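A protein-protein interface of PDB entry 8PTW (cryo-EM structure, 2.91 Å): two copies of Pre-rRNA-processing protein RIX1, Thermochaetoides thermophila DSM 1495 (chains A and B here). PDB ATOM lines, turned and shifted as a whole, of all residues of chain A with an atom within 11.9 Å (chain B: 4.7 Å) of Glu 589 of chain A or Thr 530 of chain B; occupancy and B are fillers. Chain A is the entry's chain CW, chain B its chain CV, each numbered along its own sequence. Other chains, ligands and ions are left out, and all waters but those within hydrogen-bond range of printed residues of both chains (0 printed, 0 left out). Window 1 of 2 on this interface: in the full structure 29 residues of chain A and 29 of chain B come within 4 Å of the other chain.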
ATOM      1  N   GLN A 555     -34.437  15.945 -15.823  1.00  0.00           N
ATOM      2  CA  GLN A 555     -33.085  16.427 -15.557  1.00  0.00           C
ATOM      3  C   GLN A 555     -32.509  15.801 -14.294  1.00  0.00           C
ATOM      4  O   GLN A 555     -31.329  15.433 -14.259  1.00  0.00           O
ATOM      5  CB  GLN A 555     -33.081  17.950 -15.438  1.00  0.00           C
ATOM      6  CG  GLN A 555     -31.711  18.531 -15.149  1.00  0.00           C
ATOM      7  CD  GLN A 555     -31.719  20.038 -15.057  1.00  0.00           C
ATOM      8  OE1 GLN A 555     -30.666  20.670 -15.013  1.00  0.00           O
ATOM      9  NE2 GLN A 555     -32.909  20.627 -15.032  1.00  0.00           N
ATOM     10  N   SER A 556     -33.329  15.674 -13.248  1.00  0.00           N
ATOM     11  CA  SER A 556     -32.838  15.166 -11.972  1.00  0.00           C
ATOM     12  C   SER A 556     -32.446  13.696 -12.065  1.00  0.00           C
ATOM     13  O   SER A 556     -31.408  13.291 -11.529  1.00  0.00           O
ATOM     14  CB  SER A 556     -33.893  15.378 -10.890  1.00  0.00           C
ATOM     15  OG  SER A 556     -34.435  16.684 -10.962  1.00  0.00           O
ATOM     16  N   LEU A 559     -29.242  13.434 -14.187  1.00  0.00           N
ATOM     17  CA  LEU A 559     -28.123  13.884 -13.368  1.00  0.00           C
ATOM     18  C   LEU A 559     -27.732  12.837 -12.332  1.00  0.00           C
ATOM     19  O   LEU A 559     -26.541  12.580 -12.114  1.00  0.00           O
ATOM     20  CB  LEU A 559     -28.501  15.197 -12.689  1.00  0.00           C
ATOM     21  CG  LEU A 559     -27.468  15.968 -11.880  1.00  0.00           C
ATOM     22  CD1 LEU A 559     -26.308  16.397 -12.758  1.00  0.00           C
ATOM     23  CD2 LEU A 559     -28.149  17.158 -11.243  1.00  0.00           C
ATOM     24  N   LEU A 563     -24.230  10.797 -11.845  1.00  0.00           N
ATOM     25  CA  LEU A 563     -23.426  10.817 -10.628  1.00  0.00           C
ATOM     26  C   LEU A 563     -23.325   9.462  -9.941  1.00  0.00           C
ATOM     27  O   LEU A 563     -22.497   9.310  -9.036  1.00  0.00           O
ATOM     28  CB  LEU A 563     -23.991  11.832  -9.639  1.00  0.00           C
ATOM     29  CG  LEU A 563     -24.025  13.280 -10.110  1.00  0.00           C
ATOM     30  CD1 LEU A 563     -24.527  14.138  -8.984  1.00  0.00           C
ATOM     31  CD2 LEU A 563     -22.653  13.734 -10.574  1.00  0.00           C
ATOM     32  N   LEU A 578     -24.738  11.468 -20.012  1.00  0.00           N
ATOM     33  CA  LEU A 578     -24.460  12.902 -20.077  1.00  0.00           C
ATOM     34  C   LEU A 578     -24.768  13.574 -21.420  1.00  0.00           C
ATOM     35  O   LEU A 578     -25.230  14.729 -21.384  1.00  0.00           O
ATOM     36  CB  LEU A 578     -22.998  13.145 -19.671  1.00  0.00           C
ATOM     37  CG  LEU A 578     -22.545  14.592 -19.463  1.00  0.00           C
ATOM     38  CD1 LEU A 578     -23.308  15.234 -18.320  1.00  0.00           C
ATOM     39  CD2 LEU A 578     -21.050  14.656 -19.211  1.00  0.00           C
ATOM     40  N   LEU A 581     -28.379  14.617 -21.408  1.00  0.00           N
ATOM     41  CA  LEU A 581     -28.631  15.681 -20.442  1.00  0.00           C
ATOM     42  C   LEU A 581     -28.167  17.036 -20.964  1.00  0.00           C
ATOM     43  O   LEU A 581     -28.869  18.041 -20.807  1.00  0.00           O
ATOM     44  CB  LEU A 581     -27.942  15.352 -19.118  1.00  0.00           C
ATOM     45  CG  LEU A 581     -28.071  16.384 -17.999  1.00  0.00           C
ATOM     46  CD1 LEU A 581     -29.526  16.577 -17.616  1.00  0.00           C
ATOM     47  CD2 LEU A 581     -27.248  15.969 -16.794  1.00  0.00           C
ATOM     48  N   VAL A 582     -26.986  17.087 -21.586  1.00  0.00           N
ATOM     49  CA  VAL A 582     -26.485  18.364 -22.093  1.00  0.00           C
ATOM     50  C   VAL A 582     -27.261  18.793 -23.336  1.00  0.00           C
ATOM     51  O   VAL A 582     -27.477  19.990 -23.563  1.00  0.00           O
ATOM     52  CB  VAL A 582     -24.968  18.285 -22.351  1.00  0.00           C
ATOM     53  CG1 VAL A 582     -24.417  19.648 -22.736  1.00  0.00           C
ATOM     54  CG2 VAL A 582     -24.254  17.797 -21.111  1.00  0.00           C
ATOM     55  N   ARG A 584     -30.512  18.131 -23.957  1.00  0.00           N
ATOM     56  CA  ARG A 584     -31.862  18.571 -23.619  1.00  0.00           C
ATOM     57  C   ARG A 584     -31.850  19.811 -22.725  1.00  0.00           C
ATOM     58  O   ARG A 584     -32.668  20.717 -22.916  1.00  0.00           O
ATOM     59  CB  ARG A 584     -32.634  17.417 -22.975  1.00  0.00           C
ATOM     60  CG  ARG A 584     -34.011  17.753 -22.408  1.00  0.00           C
ATOM     61  CD  ARG A 584     -34.966  18.441 -23.370  1.00  0.00           C
ATOM     62  NE  ARG A 584     -35.244  17.674 -24.575  1.00  0.00           N
ATOM     63  CZ  ARG A 584     -35.977  18.125 -25.583  1.00  0.00           C
ATOM     64  NH1 ARG A 584     -36.541  19.320 -25.546  1.00  0.00           N
ATOM     65  NH2 ARG A 584     -36.152  17.357 -26.652  1.00  0.00           N
ATOM     66  N   PHE A 585     -30.924  19.892 -21.772  1.00  0.00           N
ATOM     67  CA  PHE A 585     -30.825  21.036 -20.863  1.00  0.00           C
ATOM     68  C   PHE A 585     -29.422  21.622 -20.938  1.00  0.00           C
ATOM     69  O   PHE A 585     -28.568  21.336 -20.091  1.00  0.00           O
ATOM     70  CB  PHE A 585     -31.165  20.641 -19.426  1.00  0.00           C
ATOM     71  CG  PHE A 585     -32.463  19.905 -19.285  1.00  0.00           C
ATOM     72  CD1 PHE A 585     -33.666  20.585 -19.343  1.00  0.00           C
ATOM     73  CD2 PHE A 585     -32.480  18.538 -19.073  1.00  0.00           C
ATOM     74  CE1 PHE A 585     -34.863  19.914 -19.208  1.00  0.00           C
ATOM     75  CE2 PHE A 585     -33.675  17.861 -18.934  1.00  0.00           C
ATOM     76  CZ  PHE A 585     -34.868  18.551 -19.003  1.00  0.00           C
ATOM     77  N   PRO A 586     -29.150  22.459 -21.942  1.00  0.00           N
ATOM     78  CA  PRO A 586     -27.790  23.000 -22.079  1.00  0.00           C
ATOM     79  C   PRO A 586     -27.466  24.092 -21.077  1.00  0.00           C
ATOM     80  O   PRO A 586     -26.340  24.146 -20.570  1.00  0.00           O
ATOM     81  CB  PRO A 586     -27.772  23.536 -23.520  1.00  0.00           C
ATOM     82  CG  PRO A 586     -29.022  23.004 -24.171  1.00  0.00           C
ATOM     83  CD  PRO A 586     -30.008  22.861 -23.066  1.00  0.00           C
ATOM     84  N   ARG A 587     -28.423  24.968 -20.771  1.00  0.00           N
ATOM     85  CA  ARG A 587     -28.160  26.172 -19.994  1.00  0.00           C
ATOM     86  C   ARG A 587     -28.683  26.085 -18.565  1.00  0.00           C
ATOM     87  O   ARG A 587     -28.685  27.094 -17.852  1.00  0.00           O
ATOM     88  CB  ARG A 587     -28.762  27.386 -20.698  1.00  0.00           C
ATOM     89  CG  ARG A 587     -27.843  28.033 -21.710  1.00  0.00           C
ATOM     90  CD  ARG A 587     -28.628  28.890 -22.682  1.00  0.00           C
ATOM     91  NE  ARG A 587     -29.530  28.099 -23.509  1.00  0.00           N
ATOM     92  CZ  ARG A 587     -29.173  27.493 -24.633  1.00  0.00           C
ATOM     93  NH1 ARG A 587     -27.933  27.555 -25.087  1.00  0.00           N
ATOM     94  NH2 ARG A 587     -30.083  26.808 -25.317  1.00  0.00           N
ATOM     95  N   ASP A 588     -29.123  24.909 -18.128  1.00  0.00           N
ATOM     96  CA  ASP A 588     -29.660  24.774 -16.783  1.00  0.00           C
ATOM     97  C   ASP A 588     -28.549  24.832 -15.742  1.00  0.00           C
ATOM     98  O   ASP A 588     -27.361  24.722 -16.058  1.00  0.00           O
ATOM     99  CB  ASP A 588     -30.447  23.475 -16.644  1.00  0.00           C
ATOM    100  CG  ASP A 588     -31.856  23.588 -17.188  1.00  0.00           C
ATOM    101  OD1 ASP A 588     -32.116  24.521 -17.976  1.00  0.00           O
ATOM    102  OD2 ASP A 588     -32.706  22.750 -16.820  1.00  0.00           O
ATOM    103  N   GLU A 589     -28.954  25.011 -14.483  1.00  0.00           N
ATOM    104  CA  GLU A 589     -27.990  25.317 -13.430  1.00  0.00           C
ATOM    105  C   GLU A 589     -27.184  24.086 -13.033  1.00  0.00           C
ATOM    106  O   GLU A 589     -26.021  24.203 -12.636  1.00  0.00           O
ATOM    107  CB  GLU A 589     -28.719  25.904 -12.220  1.00  0.00           C
ATOM    108  CG  GLU A 589     -27.809  26.517 -11.163  1.00  0.00           C
ATOM    109  CD  GLU A 589     -27.073  27.748 -11.663  1.00  0.00           C
ATOM    110  OE1 GLU A 589     -27.603  28.449 -12.551  1.00  0.00           O
ATOM    111  OE2 GLU A 589     -25.964  28.022 -11.162  1.00  0.00           O
ATOM    112  N   SER A 590     -27.784  22.896 -13.134  1.00  0.00           N
ATOM    113  CA  SER A 590     -27.079  21.670 -12.765  1.00  0.00           C
ATOM    114  C   SER A 590     -25.924  21.376 -13.717  1.00  0.00           C
ATOM    115  O   SER A 590     -24.826  21.002 -13.283  1.00  0.00           O
ATOM    116  CB  SER A 590     -28.061  20.502 -12.737  1.00  0.00           C
ATOM    117  OG  SER A 590     -28.577  20.242 -14.031  1.00  0.00           O
ATOM    118  N   VAL A 591     -26.150  21.549 -15.019  1.00  0.00           N
ATOM    119  CA  VAL A 591     -25.072  21.380 -15.989  1.00  0.00           C
ATOM    120  C   VAL A 591     -24.037  22.486 -15.823  1.00  0.00           C
ATOM    121  O   VAL A 591     -22.842  22.288 -16.078  1.00  0.00           O
ATOM    122  CB  VAL A 591     -25.653  21.331 -17.415  1.00  0.00           C
ATOM    123  CG1 VAL A 591     -24.598  20.899 -18.418  1.00  0.00           C
ATOM    124  CG2 VAL A 591     -26.841  20.390 -17.456  1.00  0.00           C
ATOM    125  N   GLU A 592     -24.478  23.662 -15.367  1.00  0.00           N
ATOM    126  CA  GLU A 592     -23.544  24.735 -15.037  1.00  0.00           C
ATOM    127  C   GLU A 592     -22.656  24.352 -13.857  1.00  0.00           C
ATOM    128  O   GLU A 592     -21.477  24.725 -13.813  1.00  0.00           O
ATOM    129  CB  GLU A 592     -24.320  26.021 -14.741  1.00  0.00           C
ATOM    130  CG  GLU A 592     -23.455  27.239 -14.466  1.00  0.00           C
ATOM    131  CD  GLU A 592     -22.751  27.754 -15.700  1.00  0.00           C
ATOM    132  OE1 GLU A 592     -23.257  27.528 -16.819  1.00  0.00           O
ATOM    133  OE2 GLU A 592     -21.685  28.386 -15.548  1.00  0.00           O
ATOM    134  N   VAL A 593     -23.205  23.616 -12.887  1.00  0.00           N
ATOM    135  CA  VAL A 593     -22.390  23.117 -11.779  1.00  0.00           C
ATOM    136  C   VAL A 593     -21.431  22.043 -12.282  1.00  0.00           C
ATOM    137  O   VAL A 593     -20.277  21.960 -11.841  1.00  0.00           O
ATOM    138  CB  VAL A 593     -23.289  22.593 -10.640  1.00  0.00           C
ATOM    139  CG1 VAL A 593     -22.461  21.993  -9.533  1.00  0.00           C
ATOM    140  CG2 VAL A 593     -24.145  23.690 -10.081  1.00  0.00           C
ATOM    141  N   LEU A 594     -21.891  21.215 -13.226  1.00  0.00           N
ATOM    142  CA  LEU A 594     -21.005  20.244 -13.871  1.00  0.00           C
ATOM    143  C   LEU A 594     -19.886  20.931 -14.648  1.00  0.00           C
ATOM    144  O   LEU A 594     -18.822  20.343 -14.866  1.00  0.00           O
ATOM    145  CB  LEU A 594     -21.793  19.327 -14.809  1.00  0.00           C
ATOM    146  CG  LEU A 594     -22.747  18.279 -14.238  1.00  0.00           C
ATOM    147  CD1 LEU A 594     -23.830  17.921 -15.238  1.00  0.00           C
ATOM    148  CD2 LEU A 594     -21.972  17.041 -13.820  1.00  0.00           C
ATOM    149  N   ARG A 595     -20.112  22.174 -15.080  1.00  0.00           N
ATOM    150  CA  ARG A 595     -19.111  22.882 -15.871  1.00  0.00           C
ATOM    151  C   ARG A 595     -18.092  23.609 -15.002  1.00  0.00           C
ATOM    152  O   ARG A 595     -17.274  24.375 -15.524  1.00  0.00           O
ATOM    153  CB  ARG A 595     -19.792  23.874 -16.810  1.00  0.00           C
ATOM    154  CG  ARG A 595     -20.343  23.250 -18.069  1.00  0.00           C
ATOM    155  CD  ARG A 595     -21.168  24.250 -18.844  1.00  0.00           C
ATOM    156  NE  ARG A 595     -22.078  23.593 -19.772  1.00  0.00           N
ATOM    157  CZ  ARG A 595     -23.348  23.929 -19.934  1.00  0.00           C
ATOM    158  NH1 ARG A 595     -23.898  24.911 -19.238  1.00  0.00           N
ATOM    159  NH2 ARG A 595     -24.088  23.265 -20.816  1.00  0.00           N
ATOM    160  N   SER A 596     -18.138  23.410 -13.687  1.00  0.00           N
ATOM    161  CA  SER A 596     -17.234  24.091 -12.761  1.00  0.00           C
ATOM    162  C   SER A 596     -15.775  23.701 -12.979  1.00  0.00           C
ATOM    163  O   SER A 596     -14.868  24.309 -12.410  1.00  0.00           O
ATOM    164  CB  SER A 596     -17.627  23.787 -11.317  1.00  0.00           C
ATOM    165  OG  SER A 596     -18.912  24.299 -11.023  1.00  0.00           O
ATOM    166  N   PRO B 526     -31.519  34.209  -7.382  1.00  0.00           N
ATOM    167  CA  PRO B 526     -30.433  33.566  -8.148  1.00  0.00           C
ATOM    168  C   PRO B 526     -30.176  34.214  -9.497  1.00  0.00           C
ATOM    169  O   PRO B 526     -29.064  34.117 -10.038  1.00  0.00           O
ATOM    170  CB  PRO B 526     -30.928  32.122  -8.310  1.00  0.00           C
ATOM    171  CG  PRO B 526     -31.898  31.934  -7.228  1.00  0.00           C
ATOM    172  CD  PRO B 526     -32.595  33.236  -7.116  1.00  0.00           C
ATOM    173  N   THR B 527     -31.194  34.865 -10.059  1.00  0.00           N
ATOM    174  CA  THR B 527     -31.068  35.485 -11.369  1.00  0.00           C
ATOM    175  C   THR B 527     -30.146  36.700 -11.325  1.00  0.00           C
ATOM    176  O   THR B 527     -29.465  36.988 -12.315  1.00  0.00           O
ATOM    177  CB  THR B 527     -32.470  35.839 -11.878  1.00  0.00           C
ATOM    178  OG1 THR B 527     -33.248  34.640 -11.964  1.00  0.00           O
ATOM    179  CG2 THR B 527     -32.425  36.441 -13.256  1.00  0.00           C
ATOM    180  N   PHE B 528     -30.058  37.375 -10.175  1.00  0.00           N
ATOM    181  CA  PHE B 528     -29.136  38.497 -10.020  1.00  0.00           C
ATOM    182  C   PHE B 528     -27.683  38.048 -10.124  1.00  0.00           C
ATOM    183  O   PHE B 528     -26.802  38.838 -10.479  1.00  0.00           O
ATOM    184  CB  PHE B 528     -29.378  39.195  -8.684  1.00  0.00           C
ATOM    185  CG  PHE B 528     -30.591  40.070  -8.670  1.00  0.00           C
ATOM    186  CD1 PHE B 528     -30.896  40.863  -9.762  1.00  0.00           C
ATOM    187  CD2 PHE B 528     -31.411  40.121  -7.558  1.00  0.00           C
ATOM    188  CE1 PHE B 528     -32.007  41.679  -9.753  1.00  0.00           C
ATOM    189  CE2 PHE B 528     -32.522  40.936  -7.542  1.00  0.00           C
ATOM    190  CZ  PHE B 528     -32.818  41.719  -8.642  1.00  0.00           C
ATOM    191  N   PHE B 529     -27.406  36.788  -9.789  1.00  0.00           N
ATOM    192  CA  PHE B 529     -26.057  36.269  -9.983  1.00  0.00           C
ATOM    193  C   PHE B 529     -25.884  35.695 -11.382  1.00  0.00           C
ATOM    194  O   PHE B 529     -24.895  35.993 -12.062  1.00  0.00           O
ATOM    195  CB  PHE B 529     -25.737  35.207  -8.936  1.00  0.00           C
ATOM    196  CG  PHE B 529     -25.904  35.673  -7.523  1.00  0.00           C
ATOM    197  CD1 PHE B 529     -24.965  36.504  -6.938  1.00  0.00           C
ATOM    198  CD2 PHE B 529     -26.992  35.263  -6.770  1.00  0.00           C
ATOM    199  CE1 PHE B 529     -25.112  36.925  -5.635  1.00  0.00           C
ATOM    200  CE2 PHE B 529     -27.145  35.681  -5.468  1.00  0.00           C
ATOM    201  CZ  PHE B 529     -26.204  36.510  -4.900  1.00  0.00           C
ATOM    202  N   THR B 530     -26.832  34.867 -11.829  1.00  0.00           N
ATOM    203  CA  THR B 530     -26.646  34.135 -13.080  1.00  0.00           C
ATOM    204  C   THR B 530     -26.719  35.045 -14.300  1.00  0.00           C
ATOM    205  O   THR B 530     -25.874  34.958 -15.198  1.00  0.00           O
ATOM    206  CB  THR B 530     -27.683  33.016 -13.208  1.00  0.00           C
ATOM    207  OG1 THR B 530     -28.999  33.553 -13.048  1.00  0.00           O
ATOM    208  CG2 THR B 530     -27.447  31.942 -12.174  1.00  0.00           C
ATOM    209  N   HIS B 531     -27.716  35.923 -14.355  1.00  0.00           N
ATOM    210  CA  HIS B 531     -28.030  36.662 -15.568  1.00  0.00           C
ATOM    211  C   HIS B 531     -27.887  38.169 -15.417  1.00  0.00           C
ATOM    212  O   HIS B 531     -28.645  38.913 -16.045  1.00  0.00           O
ATOM    213  CB  HIS B 531     -29.446  36.318 -16.024  1.00  0.00           C
ATOM    214  CG  HIS B 531     -29.562  34.961 -16.642  1.00  0.00           C
ATOM    215  ND1 HIS B 531     -29.782  33.822 -15.899  1.00  0.00           N
ATOM    216  CD2 HIS B 531     -29.475  34.558 -17.931  1.00  0.00           C
ATOM    217  CE1 HIS B 531     -29.829  32.776 -16.704  1.00  0.00           C
ATOM    218  NE2 HIS B 531     -29.648  33.195 -17.942  1.00  0.00           N
ATOM    219  N   LEU B 532     -26.949  38.637 -14.605  1.00  0.00           N
ATOM    220  CA  LEU B 532     -26.649  40.052 -14.499  1.00  0.00           C
ATOM    221  C   LEU B 532     -25.144  40.245 -14.543  1.00  0.00           C
ATOM    222  O   LEU B 532     -24.411  39.399 -14.013  1.00  0.00           O
ATOM    223  CB  LEU B 532     -27.218  40.624 -13.197  1.00  0.00           C
ATOM    224  CG  LEU B 532     -27.486  42.125 -13.098  1.00  0.00           C
ATOM    225  CD1 LEU B 532     -28.538  42.547 -14.106  1.00  0.00           C
ATOM    226  CD2 LEU B 532     -27.925  42.483 -11.693  1.00  0.00           C
ATOM    227  N   LEU B 559     -25.650  28.812  -4.596  1.00  0.00           N
ATOM    228  CA  LEU B 559     -24.967  28.090  -5.664  1.00  0.00           C
ATOM    229  C   LEU B 559     -24.577  29.022  -6.807  1.00  0.00           C
ATOM    230  O   LEU B 559     -23.462  28.935  -7.338  1.00  0.00           O
ATOM    231  CB  LEU B 559     -25.873  26.972  -6.169  1.00  0.00           C
ATOM    232  CG  LEU B 559     -25.346  25.972  -7.188  1.00  0.00           C
ATOM    233  CD1 LEU B 559     -24.171  25.205  -6.622  1.00  0.00           C
ATOM    234  CD2 LEU B 559     -26.472  25.041  -7.582  1.00  0.00           C
ATOM    235  N   ALA B 560     -25.481  29.926  -7.190  1.00  0.00           N
ATOM    236  CA  ALA B 560     -25.201  30.864  -8.271  1.00  0.00           C
ATOM    237  C   ALA B 560     -24.114  31.859  -7.883  1.00  0.00           C
ATOM    238  O   ALA B 560     -23.316  32.274  -8.730  1.00  0.00           O
ATOM    239  CB  ALA B 560     -26.482  31.595  -8.661  1.00  0.00           C
ATOM    240  N   LEU B 563     -20.898  30.011  -8.280  1.00  0.00           N
ATOM    241  CA  LEU B 563     -20.478  29.814  -9.663  1.00  0.00           C
ATOM    242  C   LEU B 563     -20.171  31.110 -10.400  1.00  0.00           C
ATOM    243  O   LEU B 563     -19.614  31.053 -11.501  1.00  0.00           O
ATOM    244  CB  LEU B 563     -21.550  29.051 -10.436  1.00  0.00           C
ATOM    245  CG  LEU B 563     -21.880  27.659  -9.914  1.00  0.00           C
ATOM    246  CD1 LEU B 563     -22.874  27.010 -10.836  1.00  0.00           C
ATOM    247  CD2 LEU B 563     -20.628  26.815  -9.780  1.00  0.00           C
ATOM    248  N   HIS B 564     -20.519  32.264  -9.838  1.00  0.00           N
ATOM    249  CA  HIS B 564     -20.273  33.557 -10.474  1.00  0.00           C
ATOM    250  C   HIS B 564     -19.522  34.449  -9.497  1.00  0.00           C
ATOM    251  O   HIS B 564     -20.144  35.270  -8.800  1.00  0.00           O
ATOM    252  CB  HIS B 564     -21.575  34.217 -10.916  1.00  0.00           C
ATOM    253  CG  HIS B 564     -22.363  33.404 -11.894  1.00  0.00           C
ATOM    254  ND1 HIS B 564     -23.265  32.439 -11.503  1.00  0.00           N
ATOM    255  CD2 HIS B 564     -22.383  33.412 -13.247  1.00  0.00           C
ATOM    256  CE1 HIS B 564     -23.808  31.888 -12.574  1.00  0.00           C
ATOM    257  NE2 HIS B 564     -23.289  32.459 -13.645  1.00  0.00           N
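OG1 of Thr 530 of chain B sits at hydrogen-bond distance from ND1 of His 531 of chain B (3.0 Å).
O of Val 593 of chain A sits at hydrogen-bond distance from OG of Ser 596 of chain A, 2.8 Å away.
The side-chain carboxylate of Glu 592 of chain A is in salt-bridge range of the guanidinium group of Arg 595 of chain A (3.6 Å).
The backbone carbonyl oxygen (O) of Pro 526 of chain B lies within hydrogen-bond range of the side-chain hydroxyl (OG1) of Thr 530 of chain B (3.1 Å).
Among the printed residues, merely in contact across the chains: Glu 589 of chain A with Thr 530 of chain B (3.5 Å), Glu 589 of chain A with Leu 563 of chain B (3.3 Å), Glu 592 of chain A with Leu 563 of chain B (3.7 Å), Val 593 of chain A with Leu 559 of chain B (3.7 Å), Val 593 of chain A with Leu 563 of chain B (3.6 Å) and Ser 596 of chain A with Leu 563 of chain B (3.3 Å).
Gln 555 of chain A touches none of the printed residues of chain B.
Arg 584 of chain A touches none of the printed residues of chain B.
Of chain B, only Thr 530 (3.5 Å) and Leu 563 (3.3 Å) come within 4 Å of Glu 589 of chain A.
Of the printed residues of chain B, Glu 592 of chain A touches Leu 563 (3.7 Å).
Printed residues of chain B within 4 Å of Val 593 of chain A: Leu 559 (3.7 Å) and Leu 563 (3.6 Å).
Printed residues of chain B within 4 Å of Ser 596 of chain A: Leu 563 (3.3 Å).
No residue of chain A comes within 4 Å of Thr 527 of chain B.
Of chain A, only Glu 589 (3.5 Å) comes within 4 Å of Thr 530 of chain B.
No residue of chain A comes within 4 Å of His 531 of chain B.
Leu 532 of chain B touches none of the printed residues of chain A.
Printed residues of chain A within 4 Å of Leu 559 of chain B: Val 593.
No residue of chain A comes within 4 Å of Ala 560 of chain B.
The nearest printed residue of chain B that does not touch Glu 589 of chain A is Leu 559 of chain B (4.1 Å).
The nearest printed residue of chain B that does not touch Ser 596 of chain A is Leu 559 of chain B (6.9 Å).
Of the 11 printed residues of chain B, 3 touch a printed residue of chain A.
Printed residues of chain A that touch a printed residue of chain B: Glu 589, Glu 592, Val 593 and Ser 596.
Hydrophobic or aromatic side chains of chain A within 4 Å of the printed part of chain B: Val 593.
Along chain A the printed residues that touch a printed residue of chain B span positions 589 to 596.
Positions printed for both chains: 559 and 563.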
